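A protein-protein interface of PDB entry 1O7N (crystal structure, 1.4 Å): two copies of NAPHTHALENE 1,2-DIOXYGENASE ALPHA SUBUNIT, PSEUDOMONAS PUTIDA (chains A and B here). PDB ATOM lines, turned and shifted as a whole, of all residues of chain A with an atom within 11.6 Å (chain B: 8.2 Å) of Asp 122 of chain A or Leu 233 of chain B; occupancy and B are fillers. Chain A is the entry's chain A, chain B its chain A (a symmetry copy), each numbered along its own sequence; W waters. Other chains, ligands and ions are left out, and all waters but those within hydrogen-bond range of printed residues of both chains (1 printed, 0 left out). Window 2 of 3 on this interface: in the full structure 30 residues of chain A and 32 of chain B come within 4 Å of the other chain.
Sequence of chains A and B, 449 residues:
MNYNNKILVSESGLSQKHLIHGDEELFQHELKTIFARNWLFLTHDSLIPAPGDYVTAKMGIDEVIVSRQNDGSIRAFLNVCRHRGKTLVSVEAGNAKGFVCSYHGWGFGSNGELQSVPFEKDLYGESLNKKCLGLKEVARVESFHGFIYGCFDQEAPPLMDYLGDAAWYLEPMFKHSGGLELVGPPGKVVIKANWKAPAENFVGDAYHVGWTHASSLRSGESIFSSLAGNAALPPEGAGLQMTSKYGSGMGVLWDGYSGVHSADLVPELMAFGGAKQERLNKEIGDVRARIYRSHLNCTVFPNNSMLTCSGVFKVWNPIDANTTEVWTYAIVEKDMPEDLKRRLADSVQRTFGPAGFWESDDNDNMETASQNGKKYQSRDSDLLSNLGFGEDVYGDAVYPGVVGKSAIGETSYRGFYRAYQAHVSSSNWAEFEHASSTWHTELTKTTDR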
ATOM      1  N   HIS A 104       8.263  -3.367   1.340  1.00  0.00           N
ATOM      2  CA  HIS A 104       7.042  -4.014   0.859  1.00  0.00           C
ATOM      3  C   HIS A 104       7.165  -4.557  -0.555  1.00  0.00           C
ATOM      4  O   HIS A 104       6.177  -5.040  -1.124  1.00  0.00           O
ATOM      5  CB  HIS A 104       5.835  -3.097   0.937  1.00  0.00           C
ATOM      6  CG  HIS A 104       5.735  -2.417   2.289  1.00  0.00           C
ATOM      7  ND1 HIS A 104       6.389  -1.231   2.539  1.00  0.00           N
ATOM      8  CD2 HIS A 104       5.091  -2.736   3.440  1.00  0.00           C
ATOM      9  CE1 HIS A 104       6.157  -0.850   3.777  1.00  0.00           C
ATOM     10  NE2 HIS A 104       5.361  -1.744   4.348  1.00  0.00           N
ATOM     11  N   SER A 116       5.779  -2.755 -10.675  1.00  0.00           N
ATOM     12  CA  SER A 116       5.055  -3.809  -9.991  1.00  0.00           C
ATOM     13  C   SER A 116       4.899  -3.539  -8.525  1.00  0.00           C
ATOM     14  O   SER A 116       5.744  -2.923  -7.855  1.00  0.00           O
ATOM     15  CB  SER A 116       5.731  -5.148 -10.170  1.00  0.00           C
ATOM     16  OG  SER A 116       6.993  -5.164  -9.553  1.00  0.00           O
ATOM     17  N   VAL A 117       3.775  -3.998  -8.032  1.00  0.00           N
ATOM     18  CA  VAL A 117       3.414  -3.876  -6.655  1.00  0.00           C
ATOM     19  C   VAL A 117       2.972  -5.284  -6.236  1.00  0.00           C
ATOM     20  O   VAL A 117       2.114  -5.887  -6.900  1.00  0.00           O
ATOM     21  CB  VAL A 117       2.293  -2.822  -6.592  1.00  0.00           C
ATOM     22  CG1 VAL A 117       1.394  -2.988  -5.427  1.00  0.00           C
ATOM     23  CG2 VAL A 117       2.897  -1.412  -6.614  1.00  0.00           C
ATOM     24  N   PRO A 118       3.554  -5.862  -5.183  1.00  0.00           N
ATOM     25  CA  PRO A 118       3.138  -7.220  -4.801  1.00  0.00           C
ATOM     26  C   PRO A 118       1.645  -7.305  -4.528  1.00  0.00           C
ATOM     27  O   PRO A 118       1.046  -6.464  -3.858  1.00  0.00           O
ATOM     28  CB  PRO A 118       3.983  -7.550  -3.568  1.00  0.00           C
ATOM     29  CG  PRO A 118       5.227  -6.663  -3.774  1.00  0.00           C
ATOM     30  CD  PRO A 118       4.661  -5.357  -4.334  1.00  0.00           C
ATOM     31  N   PHE A 119       1.029  -8.340  -5.130  1.00  0.00           N
ATOM     32  CA  PHE A 119      -0.384  -8.606  -4.978  1.00  0.00           C
ATOM     33  C   PHE A 119      -1.242  -7.407  -5.323  1.00  0.00           C
ATOM     34  O   PHE A 119      -2.243  -7.163  -4.671  1.00  0.00           O
ATOM     35  CB  PHE A 119      -0.674  -9.039  -3.537  1.00  0.00           C
ATOM     36  CG  PHE A 119       0.228 -10.162  -3.061  1.00  0.00           C
ATOM     37  CD1 PHE A 119       1.095  -9.997  -1.979  1.00  0.00           C
ATOM     38  CD2 PHE A 119       0.187 -11.380  -3.704  1.00  0.00           C
ATOM     39  CE1 PHE A 119       1.897 -11.044  -1.555  1.00  0.00           C
ATOM     40  CE2 PHE A 119       0.994 -12.426  -3.290  1.00  0.00           C
ATOM     41  CZ  PHE A 119       1.848 -12.250  -2.208  1.00  0.00           C
ATOM     42  N   GLU A 120      -0.851  -6.642  -6.336  1.00  0.00           N
ATOM     43  CA  GLU A 120      -1.562  -5.418  -6.664  1.00  0.00           C
ATOM     44  C   GLU A 120      -3.062  -5.639  -6.872  1.00  0.00           C
ATOM     45  O   GLU A 120      -3.878  -4.946  -6.275  1.00  0.00           O
ATOM     46  CB  GLU A 120      -0.942  -4.747  -7.895  1.00  0.00           C
ATOM     47  CG  GLU A 120      -1.582  -3.382  -8.174  1.00  0.00           C
ATOM     48  CD  GLU A 120      -1.096  -2.706  -9.445  1.00  0.00           C
ATOM     49  OE1 GLU A 120      -1.590  -1.596  -9.719  1.00  0.00           O
ATOM     50  OE2 GLU A 120      -0.241  -3.295 -10.144  1.00  0.00           O
ATOM     51  N   LYS A 121      -3.406  -6.641  -7.674  1.00  0.00           N
ATOM     52  CA  LYS A 121      -4.818  -6.875  -7.996  1.00  0.00           C
ATOM     53  C   LYS A 121      -5.640  -7.173  -6.755  1.00  0.00           C
ATOM     54  O   LYS A 121      -6.712  -6.600  -6.563  1.00  0.00           O
ATOM     55  CB  LYS A 121      -4.945  -8.018  -9.008  1.00  0.00           C
ATOM     56  CG  LYS A 121      -6.397  -8.380  -9.400  1.00  0.00           C
ATOM     57  CD  LYS A 121      -6.931  -7.463 -10.478  1.00  0.00           C
ATOM     58  CE  LYS A 121      -6.424  -7.834 -11.884  1.00  0.00           C
ATOM     59  NZ  LYS A 121      -5.183  -7.093 -12.279  1.00  0.00           N
ATOM     60  N   ASP A 122      -5.144  -8.066  -5.910  1.00  0.00           N
ATOM     61  CA  ASP A 122      -5.865  -8.448  -4.698  1.00  0.00           C
ATOM     62  C   ASP A 122      -5.951  -7.334  -3.665  1.00  0.00           C
ATOM     63  O   ASP A 122      -6.927  -7.255  -2.924  1.00  0.00           O
ATOM     64  CB  ASP A 122      -5.205  -9.662  -4.052  1.00  0.00           C
ATOM     65  CG  ASP A 122      -5.303 -10.910  -4.920  1.00  0.00           C
ATOM     66  OD1 ASP A 122      -6.429 -11.286  -5.315  1.00  0.00           O
ATOM     67  OD2 ASP A 122      -4.314 -11.577  -5.274  1.00  0.00           O
ATOM     68  N   LEU A 123      -4.938  -6.479  -3.606  1.00  0.00           N
ATOM     69  CA  LEU A 123      -4.866  -5.481  -2.559  1.00  0.00           C
ATOM     70  C   LEU A 123      -5.373  -4.114  -2.985  1.00  0.00           C
ATOM     71  O   LEU A 123      -6.229  -3.536  -2.326  1.00  0.00           O
ATOM     72  CB  LEU A 123      -3.426  -5.359  -2.031  1.00  0.00           C
ATOM     73  CG  LEU A 123      -2.811  -6.577  -1.350  1.00  0.00           C
ATOM     74  CD1 LEU A 123      -1.334  -6.290  -1.002  1.00  0.00           C
ATOM     75  CD2 LEU A 123      -3.595  -7.052  -0.132  1.00  0.00           C
ATOM     76  N   TYR A 124      -4.882  -3.610  -4.113  1.00  0.00           N
ATOM     77  CA  TYR A 124      -5.246  -2.268  -4.573  1.00  0.00           C
ATOM     78  C   TYR A 124      -6.321  -2.304  -5.639  1.00  0.00           C
ATOM     79  O   TYR A 124      -6.947  -1.284  -5.922  1.00  0.00           O
ATOM     80  CB  TYR A 124      -4.017  -1.532  -5.138  1.00  0.00           C
ATOM     81  CG  TYR A 124      -2.952  -1.180  -4.114  1.00  0.00           C
ATOM     82  CD1 TYR A 124      -1.870  -2.023  -3.896  1.00  0.00           C
ATOM     83  CD2 TYR A 124      -3.016   0.019  -3.403  1.00  0.00           C
ATOM     84  CE1 TYR A 124      -0.898  -1.703  -2.945  1.00  0.00           C
ATOM     85  CE2 TYR A 124      -2.033   0.356  -2.455  1.00  0.00           C
ATOM     86  CZ  TYR A 124      -0.975  -0.502  -2.251  1.00  0.00           C
ATOM     87  OH  TYR A 124       0.004  -0.198  -1.318  1.00  0.00           O
ATOM     88  N   GLY A 125      -6.547  -3.475  -6.213  1.00  0.00           N
ATOM     89  CA  GLY A 125      -7.509  -3.581  -7.298  1.00  0.00           C
ATOM     90  C   GLY A 125      -6.966  -2.726  -8.421  1.00  0.00           C
ATOM     91  O   GLY A 125      -5.805  -2.877  -8.807  1.00  0.00           O
ATOM     92  N   GLU A 126      -7.782  -1.819  -8.950  1.00  0.00           N
ATOM     93  CA  GLU A 126      -7.323  -0.909  -9.998  1.00  0.00           C
ATOM     94  C   GLU A 126      -7.103   0.511  -9.469  1.00  0.00           C
ATOM     95  O   GLU A 126      -6.931   1.457 -10.250  1.00  0.00           O
ATOM     96  CB  GLU A 126      -8.333  -0.885 -11.149  1.00  0.00           C
ATOM     97  CG  GLU A 126      -8.676  -2.277 -11.671  1.00  0.00           C
ATOM     98  CD  GLU A 126      -7.643  -2.786 -12.654  1.00  0.00           C
ATOM     99  OE1 GLU A 126      -7.198  -1.976 -13.495  1.00  0.00           O
ATOM    100  OE2 GLU A 126      -7.251  -3.982 -12.581  1.00  0.00           O
ATOM    101  N   SER A 127      -7.122   0.661  -8.145  1.00  0.00           N
ATOM    102  CA  SER A 127      -7.047   1.965  -7.477  1.00  0.00           C
ATOM    103  C   SER A 127      -5.674   2.614  -7.513  1.00  0.00           C
ATOM    104  O   SER A 127      -5.569   3.828  -7.362  1.00  0.00           O
ATOM    105  CB  SER A 127      -7.440   1.814  -6.007  1.00  0.00           C
ATOM    106  OG  SER A 127      -8.794   1.419  -5.899  1.00  0.00           O
ATOM    107  N   LEU A 128      -4.621   1.806  -7.679  1.00  0.00           N
ATOM    108  CA  LEU A 128      -3.274   2.369  -7.674  1.00  0.00           C
ATOM    109  C   LEU A 128      -2.872   2.980  -9.006  1.00  0.00           C
ATOM    110  O   LEU A 128      -2.794   2.301 -10.025  1.00  0.00           O
ATOM    111  CB  LEU A 128      -2.245   1.327  -7.239  1.00  0.00           C
ATOM    112  CG  LEU A 128      -0.959   1.878  -6.625  1.00  0.00           C
ATOM    113  CD1 LEU A 128      -1.261   2.655  -5.348  1.00  0.00           C
ATOM    114  CD2 LEU A 128      -0.025   0.728  -6.348  1.00  0.00           C
ATOM    115  N   LYS A 130      -0.158   3.795 -10.744  1.00  0.00           N
ATOM    116  CA  LYS A 130       1.291   3.585 -10.785  1.00  0.00           C
ATOM    117  C   LYS A 130       1.992   4.623 -11.647  1.00  0.00           C
ATOM    118  O   LYS A 130       3.148   4.966 -11.396  1.00  0.00           O
ATOM    119  CB  LYS A 130       1.646   2.168 -11.227  1.00  0.00           C
ATOM    120  CG  LYS A 130       1.142   1.060 -10.291  1.00  0.00           C
ATOM    121  CD  LYS A 130       1.738  -0.318 -10.624  1.00  0.00           C
ATOM    122  CE  LYS A 130       1.252  -0.862 -11.967  1.00  0.00           C
ATOM    123  NZ  LYS A 130      -0.234  -0.704 -11.952  1.00  0.00           N
ATOM    124  N   ALA B 206       0.933  -5.443   7.851  1.00  0.00           N
ATOM    125  CA  ALA B 206       1.064  -6.853   7.520  1.00  0.00           C
ATOM    126  C   ALA B 206       1.674  -7.001   6.127  1.00  0.00           C
ATOM    127  O   ALA B 206       2.224  -8.048   5.818  1.00  0.00           O
ATOM    128  CB  ALA B 206      -0.285  -7.561   7.622  1.00  0.00           C
ATOM    129  N   TYR B 207       1.541  -5.985   5.279  1.00  0.00           N
ATOM    130  CA  TYR B 207       2.063  -6.008   3.907  1.00  0.00           C
ATOM    131  C   TYR B 207       3.554  -6.346   3.876  1.00  0.00           C
ATOM    132  O   TYR B 207       3.985  -7.080   2.989  1.00  0.00           O
ATOM    133  CB  TYR B 207       1.804  -4.648   3.215  1.00  0.00           C
ATOM    134  CG  TYR B 207       1.875  -4.559   1.681  1.00  0.00           C
ATOM    135  CD1 TYR B 207       1.884  -5.680   0.873  1.00  0.00           C
ATOM    136  CD2 TYR B 207       1.882  -3.319   1.062  1.00  0.00           C
ATOM    137  CE1 TYR B 207       1.918  -5.560  -0.519  1.00  0.00           C
ATOM    138  CE2 TYR B 207       1.901  -3.180  -0.314  1.00  0.00           C
ATOM    139  CZ  TYR B 207       1.916  -4.314  -1.110  1.00  0.00           C
ATOM    140  OH  TYR B 207       1.956  -4.143  -2.482  1.00  0.00           O
ATOM    141  N   SER B 226       4.331 -19.585   5.273  1.00  0.00           N
ATOM    142  CA  SER B 226       3.951 -19.740   3.878  1.00  0.00           C
ATOM    143  C   SER B 226       4.089 -18.412   3.145  1.00  0.00           C
ATOM    144  O   SER B 226       3.918 -18.340   1.933  1.00  0.00           O
ATOM    145  CB  SER B 226       2.513 -20.271   3.742  1.00  0.00           C
ATOM    146  OG  SER B 226       1.565 -19.324   4.210  1.00  0.00           O
ATOM    147  N   LEU B 227       4.327 -17.333   3.880  1.00  0.00           N
ATOM    148  CA  LEU B 227       4.386 -16.032   3.235  1.00  0.00           C
ATOM    149  C   LEU B 227       5.794 -15.718   2.707  1.00  0.00           C
ATOM    150  O   LEU B 227       5.953 -14.767   1.983  1.00  0.00           O
ATOM    151  CB  LEU B 227       3.902 -14.946   4.187  1.00  0.00           C
ATOM    152  CG  LEU B 227       2.554 -15.161   4.869  1.00  0.00           C
ATOM    153  CD1 LEU B 227       2.343 -14.059   5.890  1.00  0.00           C
ATOM    154  CD2 LEU B 227       1.387 -15.218   3.869  1.00  0.00           C
ATOM    155  N   ALA B 228       6.800 -16.527   3.038  1.00  0.00           N
ATOM    156  CA  ALA B 228       8.177 -16.161   2.676  1.00  0.00           C
ATOM    157  C   ALA B 228       8.446 -15.725   1.225  1.00  0.00           C
ATOM    158  O   ALA B 228       8.180 -16.462   0.264  1.00  0.00           O
ATOM    159  CB  ALA B 228       9.176 -17.242   3.135  1.00  0.00           C
ATOM    160  N   ASN B 230       6.974 -13.544  -0.469  1.00  0.00           N
ATOM    161  CA  ASN B 230       5.676 -13.294  -1.100  1.00  0.00           C
ATOM    162  C   ASN B 230       5.286 -14.476  -1.977  1.00  0.00           C
ATOM    163  O   ASN B 230       4.676 -14.311  -3.032  1.00  0.00           O
ATOM    164  CB  ASN B 230       5.691 -11.982  -1.878  1.00  0.00           C
ATOM    165  CG  ASN B 230       5.571 -10.788  -0.949  1.00  0.00           C
ATOM    166  OD1 ASN B 230       5.183 -10.943   0.215  1.00  0.00           O
ATOM    167  ND2 ASN B 230       5.888  -9.612  -1.466  1.00  0.00           N
ATOM    168  N   ALA B 231       5.662 -15.664  -1.531  1.00  0.00           N
ATOM    169  CA  ALA B 231       5.335 -16.874  -2.266  1.00  0.00           C
ATOM    170  C   ALA B 231       3.836 -17.094  -2.267  1.00  0.00           C
ATOM    171  O   ALA B 231       3.301 -17.750  -3.161  1.00  0.00           O
ATOM    172  CB  ALA B 231       6.016 -18.054  -1.607  1.00  0.00           C
ATOM    173  N   ALA B 232       3.172 -16.565  -1.246  1.00  0.00           N
ATOM    174  CA  ALA B 232       1.745 -16.749  -1.080  1.00  0.00           C
ATOM    175  C   ALA B 232       1.144 -15.557  -0.334  1.00  0.00           C
ATOM    176  O   ALA B 232       1.835 -14.872   0.433  1.00  0.00           O
ATOM    177  CB  ALA B 232       1.471 -18.068  -0.330  1.00  0.00           C
ATOM    178  N   LEU B 233      -0.133 -15.296  -0.605  1.00  0.00           N
ATOM    179  CA  LEU B 233      -0.902 -14.263   0.070  1.00  0.00           C
ATOM    180  C   LEU B 233      -1.898 -14.961   1.000  1.00  0.00           C
ATOM    181  O   LEU B 233      -2.455 -15.999   0.642  1.00  0.00           O
ATOM    182  CB  LEU B 233      -1.667 -13.441  -0.971  1.00  0.00           C
ATOM    183  CG  LEU B 233      -2.467 -12.214  -0.534  1.00  0.00           C
ATOM    184  CD1 LEU B 233      -1.529 -11.095  -0.113  1.00  0.00           C
ATOM    185  CD2 LEU B 233      -3.402 -11.755  -1.661  1.00  0.00           C
ATOM    186  N   PRO B 234      -2.100 -14.417   2.196  1.00  0.00           N
ATOM    187  CA  PRO B 234      -3.097 -14.964   3.119  1.00  0.00           C
ATOM    188  C   PRO B 234      -4.437 -15.145   2.406  1.00  0.00           C
ATOM    189  O   PRO B 234      -4.785 -14.379   1.500  1.00  0.00           O
ATOM    190  CB  PRO B 234      -3.210 -13.880   4.198  1.00  0.00           C
ATOM    191  CG  PRO B 234      -1.872 -13.185   4.188  1.00  0.00           C
ATOM    192  CD  PRO B 234      -1.395 -13.257   2.766  1.00  0.00           C
ATOM    193  N   PRO B 235      -5.163 -16.142   2.948  1.00  0.00           N
ATOM    194  CA  PRO B 235      -6.538 -16.490   2.520  1.00  0.00           C
ATOM    195  C   PRO B 235      -7.604 -15.418   2.541  1.00  0.00           C
ATOM    196  O   PRO B 235      -7.339 -14.237   2.715  1.00  0.00           O
ATOM    197  CB  PRO B 235      -6.850 -17.697   3.368  1.00  0.00           C
ATOM    198  CG  PRO B 235      -5.515 -18.392   3.365  1.00  0.00           C
ATOM    199  CD  PRO B 235      -4.421 -17.395   3.148  1.00  0.00           C
ATOM    200  N   GLU B 236      -8.814 -15.895   2.352  1.00  0.00           N
ATOM    201  CA  GLU B 236     -10.071 -15.168   2.414  1.00  0.00           C
ATOM    202  C   GLU B 236     -10.052 -14.039   3.434  1.00  0.00           C
ATOM    203  O   GLU B 236      -9.391 -13.014   3.288  1.00  0.00           O
ATOM    204  CB  GLU B 236     -11.140 -16.169   2.843  1.00  0.00           C
ATOM    205  CG  GLU B 236     -10.565 -17.453   3.466  1.00  0.00           C
ATOM    206  CD  GLU B 236     -10.150 -17.339   4.950  1.00  0.00           C
ATOM    207  OE1 GLU B 236      -8.967 -17.054   5.222  1.00  0.00           O
ATOM    208  OE2 GLU B 236     -11.019 -17.537   5.803  1.00  0.00           O
ATOM    209  N   ALA B 238      -8.539 -14.005   6.210  1.00  0.00           N
ATOM    210  CA  ALA B 238      -7.513 -14.520   7.113  1.00  0.00           C
ATOM    211  C   ALA B 238      -7.306 -13.566   8.278  1.00  0.00           C
ATOM    212  O   ALA B 238      -6.699 -13.934   9.267  1.00  0.00           O
ATOM    213  CB  ALA B 238      -6.193 -14.708   6.371  1.00  0.00           C
ATOM    214  N   LEU B 387      -3.683   2.160   1.044  1.00  0.00           N
ATOM    215  CA  LEU B 387      -4.131   0.803   0.725  1.00  0.00           C
ATOM    216  C   LEU B 387      -5.400   0.518   1.512  1.00  0.00           C
ATOM    217  O   LEU B 387      -5.410   0.625   2.737  1.00  0.00           O
ATOM    218  CB  LEU B 387      -3.018  -0.209   1.039  1.00  0.00           C
ATOM    219  CG  LEU B 387      -3.374  -1.682   0.901  1.00  0.00           C
ATOM    220  CD1 LEU B 387      -3.888  -1.977  -0.512  1.00  0.00           C
ATOM    221  CD2 LEU B 387      -2.170  -2.513   1.197  1.00  0.00           C
ATOM    222  N   GLU B 391     -12.819   1.218   1.615  1.00  0.00           N
ATOM    223  CA  GLU B 391     -13.398  -0.080   1.955  1.00  0.00           C
ATOM    224  C   GLU B 391     -13.501  -0.296   3.464  1.00  0.00           C
ATOM    225  O   GLU B 391     -13.884  -1.365   3.899  1.00  0.00           O
ATOM    226  CB  GLU B 391     -12.621  -1.248   1.311  1.00  0.00           C
ATOM    227  CG  GLU B 391     -12.558  -1.213  -0.211  1.00  0.00           C
ATOM    228  CD  GLU B 391     -11.650  -2.296  -0.777  1.00  0.00           C
ATOM    229  OE1 GLU B 391     -12.095  -3.470  -0.863  1.00  0.00           O
ATOM    230  OE2 GLU B 391     -10.490  -1.976  -1.128  1.00  0.00           O
ATOM    231  N   SER B 406      -9.959  -7.182   5.928  1.00  0.00           N
ATOM    232  CA  SER B 406      -8.959  -7.882   5.120  1.00  0.00           C
ATOM    233  C   SER B 406      -7.721  -7.921   5.967  1.00  0.00           C
ATOM    234  O   SER B 406      -7.498  -7.030   6.780  1.00  0.00           O
ATOM    235  CB  SER B 406      -8.661  -7.112   3.840  1.00  0.00           C
ATOM    236  OG  SER B 406      -8.472  -5.744   4.128  1.00  0.00           O
ATOM    237  N   ALA B 407      -6.897  -8.940   5.758  1.00  0.00           N
ATOM    238  CA  ALA B 407      -5.700  -9.091   6.561  1.00  0.00           C
ATOM    239  C   ALA B 407      -4.626  -8.059   6.311  1.00  0.00           C
ATOM    240  O   ALA B 407      -3.884  -7.693   7.231  1.00  0.00           O
ATOM    241  CB  ALA B 407      -5.095 -10.498   6.359  1.00  0.00           C
ATOM    242  N   ILE B 408      -4.529  -7.607   5.075  1.00  0.00           N
ATOM    243  CA  ILE B 408      -3.473  -6.690   4.672  1.00  0.00           C
ATOM    244  C   ILE B 408      -4.013  -5.370   4.166  1.00  0.00           C
ATOM    245  O   ILE B 408      -4.772  -5.308   3.199  1.00  0.00           O
ATOM    246  CB  ILE B 408      -2.594  -7.353   3.577  1.00  0.00           C
ATOM    247  CG1 ILE B 408      -1.955  -8.634   4.109  1.00  0.00           C
ATOM    248  CG2 ILE B 408      -1.541  -6.343   3.073  1.00  0.00           C
ATOM    249  CD1 ILE B 408      -1.428  -9.534   2.994  1.00  0.00           C
HETATM  250  O   HOH W   1       5.153  -7.153   0.147  1.00  0.00           O
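The side-chain hydroxyl (OH) of Tyr 207 of chain B is in hydrogen-bond range of the backbone carbonyl oxygen (O) of Pro 118 of chain A, 2.8 Å away.
The backbone carbonyl oxygen (O) of Tyr 124 of chain A sits close to the side-chain hydroxyl (OG) of Ser 127 of chain A, at 3.3 Å.
Among the printed residues, merely in contact across the chains: Val 117 of chain A with Tyr 207 of chain B (3.2 Å), Leu 123 of chain A with Leu 387 of chain B (3.3 Å), Leu 123 of chain A with Tyr 207 of chain B (3.4 Å), Phe 119 of chain A with Leu 233 of chain B (3.4 Å), Pro 118 of chain A with Asn 230 of chain B (3.5 Å), Tyr 124 of chain A with Leu 387 of chain B (3.6 Å), Phe 119 of chain A with Asn 230 of chain B (3.6 Å), Asp 122 of chain A with Leu 233 of chain B (3.7 Å), Tyr 124 of chain A with Tyr 207 of chain B (3.7 Å), Phe 119 of chain A with Ala 232 of chain B (3.7 Å), His 104 of chain A with Tyr 207 of chain B (3.8 Å) and Leu 123 of chain A with Ile 408 of chain B (3.9 Å).
Of the printed residues of chain B, Asp 122 of chain A touches Leu 233.
Printed residues of chain B within 4 Å of Leu 123 of chain A: Tyr 207, Leu 387 and Ile 408.
No residue of chain A comes within 4 Å of Leu 227 of chain B.
No residue of chain A comes within 4 Å of Ala 231 of chain B.
Leu 233 of chain B touches two residues of chain A.
No residue of chain A comes within 4 Å of Pro 234 of chain B.
Printed residues of chain A within 4 Å of Ile 408 of chain B: Leu 123 (3.9 Å).
The nearest residue of chain A that does not touch Leu 233 of chain B is Leu 123 of chain A (4.5 Å).
The nearest printed residue of chain A that does not touch Ile 408 of chain B is Phe 119 of chain A (5.6 Å).
Hydrophobic or aromatic side chains of chain A within 4 Å of the printed part of chain B: His 104, Val 117, Pro 118, Phe 119, Leu 123 and Tyr 124.
Printed residues of chain B that touch a printed residue of chain A: Tyr 207, Asn 230, Ala 232, Leu 233, Leu 387 and Ile 408.
Along chain B the printed residues that touch a printed residue of chain A span positions 207 to 408.
Among the printed residues, no Asp or Glu carboxylate lies within 4 Å of a Lys or Arg side-chain nitrogen of the other chain.
No position is printed for both chains.
Of the 13 pairs that touch across the chains among the printed residues, none has its exchanged pair printed and touching as well.
Water W1 lies within hydrogen-bond range of O of His 104 of chain A, ND2 of Asn 230 of chain B and O of Tyr 207 of chain B.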
